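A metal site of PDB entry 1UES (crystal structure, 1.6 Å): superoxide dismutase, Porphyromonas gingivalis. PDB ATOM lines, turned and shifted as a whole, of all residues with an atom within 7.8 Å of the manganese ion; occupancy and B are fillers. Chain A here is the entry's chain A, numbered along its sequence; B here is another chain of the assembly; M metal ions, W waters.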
ATOM      1  N   HIS A  27     -18.387 -16.311 -24.188  1.00  0.00           N
ATOM      2  CA  HIS A  27     -19.066 -17.034 -23.115  1.00  0.00           C
ATOM      3  C   HIS A  27     -20.584 -16.933 -23.250  1.00  0.00           C
ATOM      4  O   HIS A  27     -21.290 -17.952 -23.270  1.00  0.00           O
ATOM      5  CB  HIS A  27     -18.594 -16.487 -21.748  1.00  0.00           C
ATOM      6  CG  HIS A  27     -18.842 -17.431 -20.618  1.00  0.00           C
ATOM      7  ND1 HIS A  27     -18.424 -17.183 -19.331  1.00  0.00           N
ATOM      8  CD2 HIS A  27     -19.420 -18.645 -20.603  1.00  0.00           C
ATOM      9  CE1 HIS A  27     -18.736 -18.206 -18.567  1.00  0.00           C
ATOM     10  NE2 HIS A  27     -19.336 -19.107 -19.322  1.00  0.00           N
ATOM     11  N   HIS A  28     -21.075 -15.708 -23.317  1.00  0.00           N
ATOM     12  CA  HIS A  28     -22.495 -15.485 -23.472  1.00  0.00           C
ATOM     13  C   HIS A  28     -22.931 -15.634 -24.928  1.00  0.00           C
ATOM     14  O   HIS A  28     -23.858 -16.375 -25.234  1.00  0.00           O
ATOM     15  CB  HIS A  28     -22.885 -14.093 -22.953  1.00  0.00           C
ATOM     16  CG  HIS A  28     -24.290 -13.692 -23.273  1.00  0.00           C
ATOM     17  ND1 HIS A  28     -24.620 -13.019 -24.427  1.00  0.00           N
ATOM     18  CD2 HIS A  28     -25.462 -13.958 -22.639  1.00  0.00           C
ATOM     19  CE1 HIS A  28     -25.932 -12.896 -24.494  1.00  0.00           C
ATOM     20  NE2 HIS A  28     -26.465 -13.455 -23.424  1.00  0.00           N
ATOM     21  N   HIS A  31     -20.999 -19.786 -26.282  1.00  0.00           N
ATOM     22  CA  HIS A  31     -21.266 -20.954 -25.434  1.00  0.00           C
ATOM     23  C   HIS A  31     -22.707 -21.055 -25.002  1.00  0.00           C
ATOM     24  O   HIS A  31     -23.338 -22.124 -25.144  1.00  0.00           O
ATOM     25  CB  HIS A  31     -20.404 -20.935 -24.188  1.00  0.00           C
ATOM     26  CG  HIS A  31     -18.965 -21.226 -24.454  1.00  0.00           C
ATOM     27  ND1 HIS A  31     -18.429 -22.485 -24.399  1.00  0.00           N
ATOM     28  CD2 HIS A  31     -17.939 -20.394 -24.753  1.00  0.00           C
ATOM     29  CE1 HIS A  31     -17.145 -22.426 -24.647  1.00  0.00           C
ATOM     30  NE2 HIS A  31     -16.815 -21.167 -24.872  1.00  0.00           N
ATOM     31  N   LEU A  32     -23.229 -19.991 -24.406  1.00  0.00           N
ATOM     32  CA  LEU A  32     -24.618 -20.047 -23.950  1.00  0.00           C
ATOM     33  C   LEU A  32     -25.583 -20.223 -25.124  1.00  0.00           C
ATOM     34  O   LEU A  32     -26.539 -20.972 -25.032  1.00  0.00           O
ATOM     35  CB  LEU A  32     -24.969 -18.833 -23.102  1.00  0.00           C
ATOM     36  CG  LEU A  32     -26.365 -18.777 -22.478  1.00  0.00           C
ATOM     37  CD1 LEU A  32     -26.690 -20.093 -21.724  1.00  0.00           C
ATOM     38  CD2 LEU A  32     -26.421 -17.608 -21.507  1.00  0.00           C
ATOM     39  N   TYR A  35     -25.691 -23.844 -25.900  1.00  0.00           N
ATOM     40  CA  TYR A  35     -26.430 -24.620 -24.895  1.00  0.00           C
ATOM     41  C   TYR A  35     -27.928 -24.496 -25.130  1.00  0.00           C
ATOM     42  O   TYR A  35     -28.659 -25.496 -25.033  1.00  0.00           O
ATOM     43  CB  TYR A  35     -26.120 -24.122 -23.481  1.00  0.00           C
ATOM     44  CG  TYR A  35     -24.760 -24.533 -22.994  1.00  0.00           C
ATOM     45  CD1 TYR A  35     -24.334 -25.858 -23.120  1.00  0.00           C
ATOM     46  CD2 TYR A  35     -23.883 -23.598 -22.448  1.00  0.00           C
ATOM     47  CE1 TYR A  35     -23.066 -26.255 -22.697  1.00  0.00           C
ATOM     48  CE2 TYR A  35     -22.598 -24.002 -22.022  1.00  0.00           C
ATOM     49  CZ  TYR A  35     -22.212 -25.315 -22.147  1.00  0.00           C
ATOM     50  OH  TYR A  35     -20.988 -25.750 -21.705  1.00  0.00           O
ATOM     51  N   GLN A  70     -26.664 -26.329 -17.957  1.00  0.00           N
ATOM     52  CA  GLN A  70     -25.771 -25.255 -18.404  1.00  0.00           C
ATOM     53  C   GLN A  70     -26.551 -23.973 -18.680  1.00  0.00           C
ATOM     54  O   GLN A  70     -26.086 -22.884 -18.341  1.00  0.00           O
ATOM     55  CB  GLN A  70     -24.967 -25.677 -19.632  1.00  0.00           C
ATOM     56  CG  GLN A  70     -23.778 -26.608 -19.305  1.00  0.00           C
ATOM     57  CD  GLN A  70     -22.783 -25.994 -18.305  1.00  0.00           C
ATOM     58  OE1 GLN A  70     -23.050 -25.965 -17.104  1.00  0.00           O
ATOM     59  NE2 GLN A  70     -21.652 -25.524 -18.799  1.00  0.00           N
ATOM     60  N   ASN A  73     -27.500 -22.538 -15.246  1.00  0.00           N
ATOM     61  CA  ASN A  73     -26.330 -22.067 -14.545  1.00  0.00           C
ATOM     62  C   ASN A  73     -25.886 -20.715 -15.129  1.00  0.00           C
ATOM     63  O   ASN A  73     -25.591 -19.779 -14.397  1.00  0.00           O
ATOM     64  CB  ASN A  73     -25.154 -23.074 -14.650  1.00  0.00           C
ATOM     65  CG  ASN A  73     -25.256 -24.218 -13.639  1.00  0.00           C
ATOM     66  OD1 ASN A  73     -25.635 -23.984 -12.501  1.00  0.00           O
ATOM     67  ND2 ASN A  73     -24.921 -25.444 -14.058  1.00  0.00           N
ATOM     68  N   HIS A  74     -25.822 -20.627 -16.454  1.00  0.00           N
ATOM     69  CA  HIS A  74     -25.361 -19.376 -17.048  1.00  0.00           C
ATOM     70  C   HIS A  74     -26.344 -18.266 -16.862  1.00  0.00           C
ATOM     71  O   HIS A  74     -25.937 -17.127 -16.686  1.00  0.00           O
ATOM     72  CB  HIS A  74     -25.062 -19.568 -18.537  1.00  0.00           C
ATOM     73  CG  HIS A  74     -23.823 -20.372 -18.775  1.00  0.00           C
ATOM     74  ND1 HIS A  74     -23.831 -21.741 -18.840  1.00  0.00           N
ATOM     75  CD2 HIS A  74     -22.537 -19.998 -18.895  1.00  0.00           C
ATOM     76  CE1 HIS A  74     -22.609 -22.189 -18.999  1.00  0.00           C
ATOM     77  NE2 HIS A  74     -21.784 -21.152 -19.036  1.00  0.00           N
ATOM     78  N   TYR A  77     -25.690 -17.050 -13.478  1.00  0.00           N
ATOM     79  CA  TYR A  77     -24.354 -16.508 -13.414  1.00  0.00           C
ATOM     80  C   TYR A  77     -24.270 -15.103 -14.022  1.00  0.00           C
ATOM     81  O   TYR A  77     -23.855 -14.141 -13.376  1.00  0.00           O
ATOM     82  CB  TYR A  77     -23.412 -17.506 -14.117  1.00  0.00           C
ATOM     83  CG  TYR A  77     -21.998 -17.027 -14.366  1.00  0.00           C
ATOM     84  CD1 TYR A  77     -21.020 -17.161 -13.384  1.00  0.00           C
ATOM     85  CD2 TYR A  77     -21.610 -16.565 -15.633  1.00  0.00           C
ATOM     86  CE1 TYR A  77     -19.682 -16.846 -13.656  1.00  0.00           C
ATOM     87  CE2 TYR A  77     -20.268 -16.261 -15.918  1.00  0.00           C
ATOM     88  CZ  TYR A  77     -19.312 -16.407 -14.916  1.00  0.00           C
ATOM     89  OH  TYR A  77     -17.972 -16.249 -15.209  1.00  0.00           O
ATOM     90  N   PHE A  78     -24.716 -14.938 -15.252  1.00  0.00           N
ATOM     91  CA  PHE A  78     -24.588 -13.612 -15.833  1.00  0.00           C
ATOM     92  C   PHE A  78     -25.474 -12.595 -15.152  1.00  0.00           C
ATOM     93  O   PHE A  78     -25.105 -11.443 -15.053  1.00  0.00           O
ATOM     94  CB  PHE A  78     -24.912 -13.628 -17.322  1.00  0.00           C
ATOM     95  CG  PHE A  78     -23.865 -14.320 -18.155  1.00  0.00           C
ATOM     96  CD1 PHE A  78     -24.194 -15.475 -18.850  1.00  0.00           C
ATOM     97  CD2 PHE A  78     -22.557 -13.829 -18.197  1.00  0.00           C
ATOM     98  CE1 PHE A  78     -23.242 -16.145 -19.590  1.00  0.00           C
ATOM     99  CE2 PHE A  78     -21.585 -14.516 -18.947  1.00  0.00           C
ATOM    100  CZ  PHE A  78     -21.942 -15.655 -19.626  1.00  0.00           C
ATOM    101  N   GLY A 122     -16.827 -27.298 -14.077  1.00  0.00           N
ATOM    102  CA  GLY A 122     -17.911 -27.300 -13.133  1.00  0.00           C
ATOM    103  C   GLY A 122     -18.248 -25.935 -12.584  1.00  0.00           C
ATOM    104  O   GLY A 122     -17.834 -24.907 -13.155  1.00  0.00           O
ATOM    105  N   TRP A 123     -18.986 -25.936 -11.479  1.00  0.00           N
ATOM    106  CA  TRP A 123     -19.462 -24.721 -10.819  1.00  0.00           C
ATOM    107  C   TRP A 123     -19.368 -24.824  -9.313  1.00  0.00           C
ATOM    108  O   TRP A 123     -19.597 -25.909  -8.776  1.00  0.00           O
ATOM    109  CB  TRP A 123     -20.932 -24.495 -11.117  1.00  0.00           C
ATOM    110  CG  TRP A 123     -21.281 -24.521 -12.559  1.00  0.00           C
ATOM    111  CD1 TRP A 123     -21.384 -25.621 -13.365  1.00  0.00           C
ATOM    112  CD2 TRP A 123     -21.535 -23.380 -13.389  1.00  0.00           C
ATOM    113  NE1 TRP A 123     -21.697 -25.239 -14.654  1.00  0.00           N
ATOM    114  CE2 TRP A 123     -21.799 -23.876 -14.696  1.00  0.00           C
ATOM    115  CE3 TRP A 123     -21.590 -21.995 -13.176  1.00  0.00           C
ATOM    116  CZ2 TRP A 123     -22.097 -23.031 -15.769  1.00  0.00           C
ATOM    117  CZ3 TRP A 123     -21.893 -21.153 -14.257  1.00  0.00           C
ATOM    118  CH2 TRP A 123     -22.140 -21.682 -15.530  1.00  0.00           C
ATOM    119  N   ASP A 157     -18.414 -19.906 -12.186  1.00  0.00           N
ATOM    120  CA  ASP A 157     -18.208 -20.888 -13.248  1.00  0.00           C
ATOM    121  C   ASP A 157     -16.718 -21.224 -13.295  1.00  0.00           C
ATOM    122  O   ASP A 157     -15.888 -20.304 -13.457  1.00  0.00           O
ATOM    123  CB  ASP A 157     -18.629 -20.222 -14.550  1.00  0.00           C
ATOM    124  CG  ASP A 157     -18.662 -21.157 -15.727  1.00  0.00           C
ATOM    125  OD1 ASP A 157     -18.357 -22.349 -15.567  1.00  0.00           O
ATOM    126  OD2 ASP A 157     -19.013 -20.614 -16.815  1.00  0.00           O
ATOM    127  N   VAL A 158     -16.363 -22.508 -13.133  1.00  0.00           N
ATOM    128  CA  VAL A 158     -14.955 -22.854 -13.205  1.00  0.00           C
ATOM    129  C   VAL A 158     -14.629 -23.677 -14.431  1.00  0.00           C
ATOM    130  O   VAL A 158     -13.577 -24.316 -14.508  1.00  0.00           O
ATOM    131  CB  VAL A 158     -14.382 -23.465 -11.881  1.00  0.00           C
ATOM    132  CG1 VAL A 158     -14.572 -22.428 -10.743  1.00  0.00           C
ATOM    133  CG2 VAL A 158     -15.077 -24.785 -11.527  1.00  0.00           C
ATOM    134  N   TRP A 159     -15.548 -23.612 -15.399  1.00  0.00           N
ATOM    135  CA  TRP A 159     -15.272 -24.208 -16.703  1.00  0.00           C
ATOM    136  C   TRP A 159     -14.163 -23.245 -17.168  1.00  0.00           C
ATOM    137  O   TRP A 159     -14.249 -22.051 -16.941  1.00  0.00           O
ATOM    138  CB  TRP A 159     -16.469 -24.056 -17.652  1.00  0.00           C
ATOM    139  CG  TRP A 159     -17.464 -25.169 -17.516  1.00  0.00           C
ATOM    140  CD1 TRP A 159     -18.216 -25.453 -16.423  1.00  0.00           C
ATOM    141  CD2 TRP A 159     -17.813 -26.119 -18.513  1.00  0.00           C
ATOM    142  NE1 TRP A 159     -19.027 -26.543 -16.666  1.00  0.00           N
ATOM    143  CE2 TRP A 159     -18.804 -26.982 -17.948  1.00  0.00           C
ATOM    144  CE3 TRP A 159     -17.394 -26.337 -19.840  1.00  0.00           C
ATOM    145  CZ2 TRP A 159     -19.375 -28.050 -18.677  1.00  0.00           C
ATOM    146  CZ3 TRP A 159     -17.980 -27.407 -20.571  1.00  0.00           C
ATOM    147  CH2 TRP A 159     -18.956 -28.253 -19.970  1.00  0.00           C
ATOM    148  N   GLU A 160     -13.097 -23.789 -17.747  1.00  0.00           N
ATOM    149  CA  GLU A 160     -11.998 -22.926 -18.175  1.00  0.00           C
ATOM    150  C   GLU A 160     -12.376 -21.817 -19.133  1.00  0.00           C
ATOM    151  O   GLU A 160     -11.753 -20.754 -19.113  1.00  0.00           O
ATOM    152  CB  GLU A 160     -10.878 -23.799 -18.766  1.00  0.00           C
ATOM    153  CG  GLU A 160     -10.247 -24.697 -17.700  1.00  0.00           C
ATOM    154  CD  GLU A 160      -9.156 -25.592 -18.250  1.00  0.00           C
ATOM    155  OE1 GLU A 160      -9.407 -26.248 -19.290  1.00  0.00           O
ATOM    156  OE2 GLU A 160      -8.055 -25.624 -17.662  1.00  0.00           O
ATOM    157  N   HIS A 161     -13.398 -22.014 -19.961  1.00  0.00           N
ATOM    158  CA  HIS A 161     -13.797 -20.957 -20.888  1.00  0.00           C
ATOM    159  C   HIS A 161     -14.267 -19.671 -20.163  1.00  0.00           C
ATOM    160  O   HIS A 161     -14.285 -18.611 -20.724  1.00  0.00           O
ATOM    161  CB  HIS A 161     -14.892 -21.457 -21.870  1.00  0.00           C
ATOM    162  CG  HIS A 161     -16.198 -21.812 -21.224  1.00  0.00           C
ATOM    163  ND1 HIS A 161     -16.759 -23.060 -21.354  1.00  0.00           N
ATOM    164  CD2 HIS A 161     -17.082 -21.078 -20.502  1.00  0.00           C
ATOM    165  CE1 HIS A 161     -17.930 -23.092 -20.749  1.00  0.00           C
ATOM    166  NE2 HIS A 161     -18.151 -21.901 -20.225  1.00  0.00           N
ATOM    167  N   ALA A 162     -14.608 -19.771 -18.881  1.00  0.00           N
ATOM    168  CA  ALA A 162     -15.063 -18.624 -18.140  1.00  0.00           C
ATOM    169  C   ALA A 162     -13.940 -17.655 -17.830  1.00  0.00           C
ATOM    170  O   ALA A 162     -14.177 -16.512 -17.590  1.00  0.00           O
ATOM    171  CB  ALA A 162     -15.725 -19.080 -16.847  1.00  0.00           C
ATOM    172  N   TYR A 163     -12.696 -18.118 -17.898  1.00  0.00           N
ATOM    173  CA  TYR A 163     -11.616 -17.237 -17.478  1.00  0.00           C
ATOM    174  C   TYR A 163     -10.331 -17.398 -18.257  1.00  0.00           C
ATOM    175  O   TYR A 163      -9.423 -16.605 -18.081  1.00  0.00           O
ATOM    176  CB  TYR A 163     -11.310 -17.501 -15.971  1.00  0.00           C
ATOM    177  CG  TYR A 163     -10.929 -18.940 -15.605  1.00  0.00           C
ATOM    178  CD1 TYR A 163      -9.609 -19.413 -15.805  1.00  0.00           C
ATOM    179  CD2 TYR A 163     -11.860 -19.840 -15.101  1.00  0.00           C
ATOM    180  CE1 TYR A 163      -9.252 -20.734 -15.518  1.00  0.00           C
ATOM    181  CE2 TYR A 163     -11.536 -21.155 -14.804  1.00  0.00           C
ATOM    182  CZ  TYR A 163     -10.212 -21.608 -15.013  1.00  0.00           C
ATOM    183  OH  TYR A 163      -9.817 -22.872 -14.669  1.00  0.00           O
ATOM    184  N   GLU B 160     -10.645 -27.471 -22.135  1.00  0.00           N
ATOM    185  CA  GLU B 160     -10.633 -26.222 -22.889  1.00  0.00           C
ATOM    186  C   GLU B 160      -9.290 -25.512 -22.969  1.00  0.00           C
ATOM    187  O   GLU B 160      -9.044 -24.796 -23.942  1.00  0.00           O
ATOM    188  CB  GLU B 160     -11.747 -25.313 -22.351  1.00  0.00           C
ATOM    189  CG  GLU B 160     -13.145 -25.919 -22.583  1.00  0.00           C
ATOM    190  CD  GLU B 160     -14.245 -25.047 -22.032  1.00  0.00           C
ATOM    191  OE1 GLU B 160     -14.151 -24.674 -20.843  1.00  0.00           O
ATOM    192  OE2 GLU B 160     -15.188 -24.725 -22.798  1.00  0.00           O
HETATM  193 MN    MN M   1     -19.616 -21.193 -18.704  1.00  0.00          MN
HETATM  194  O   HOH W   1     -19.855 -23.236 -17.820  1.00  0.00           O
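The side-chain carboxylate (OD1) of Asp 157 lies within hydrogen-bond range of the backbone NH (N) of Trp 159 (3.1 Å). The backbone carbonyl oxygen (O) of His 27 sits at hydrogen-bond distance from the backbone NH (N) of Leu 32. A ring nitrogen (ND1) of His 74 lies within hydrogen-bond range of the backbone carbonyl oxygen (O) of Gln 70, at 2.6 Å. A ring nitrogen (ND1) of His 161 is in hydrogen-bond range of the side-chain carboxylate of Glu 160 of chain B, at 2.7 Å.
The nearest printed residue that does not touch the manganese ion is Trp 123 (4.1 Å).
The manganese ion is bound by OD2 of Asp 157 (2.1 Å), NE2 of His 27 (2.2 Å), NE2 of His 74 (2.2 Å), NE2 of His 161 (2.2 Å) and water W1 (2.2 Å).
Water W1 lies within hydrogen-bond range of the side-chain carboxylate of Asp 157 (2.8 Å) and the side-chain amide nitrogen of Gln 70 (3.1 Å).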
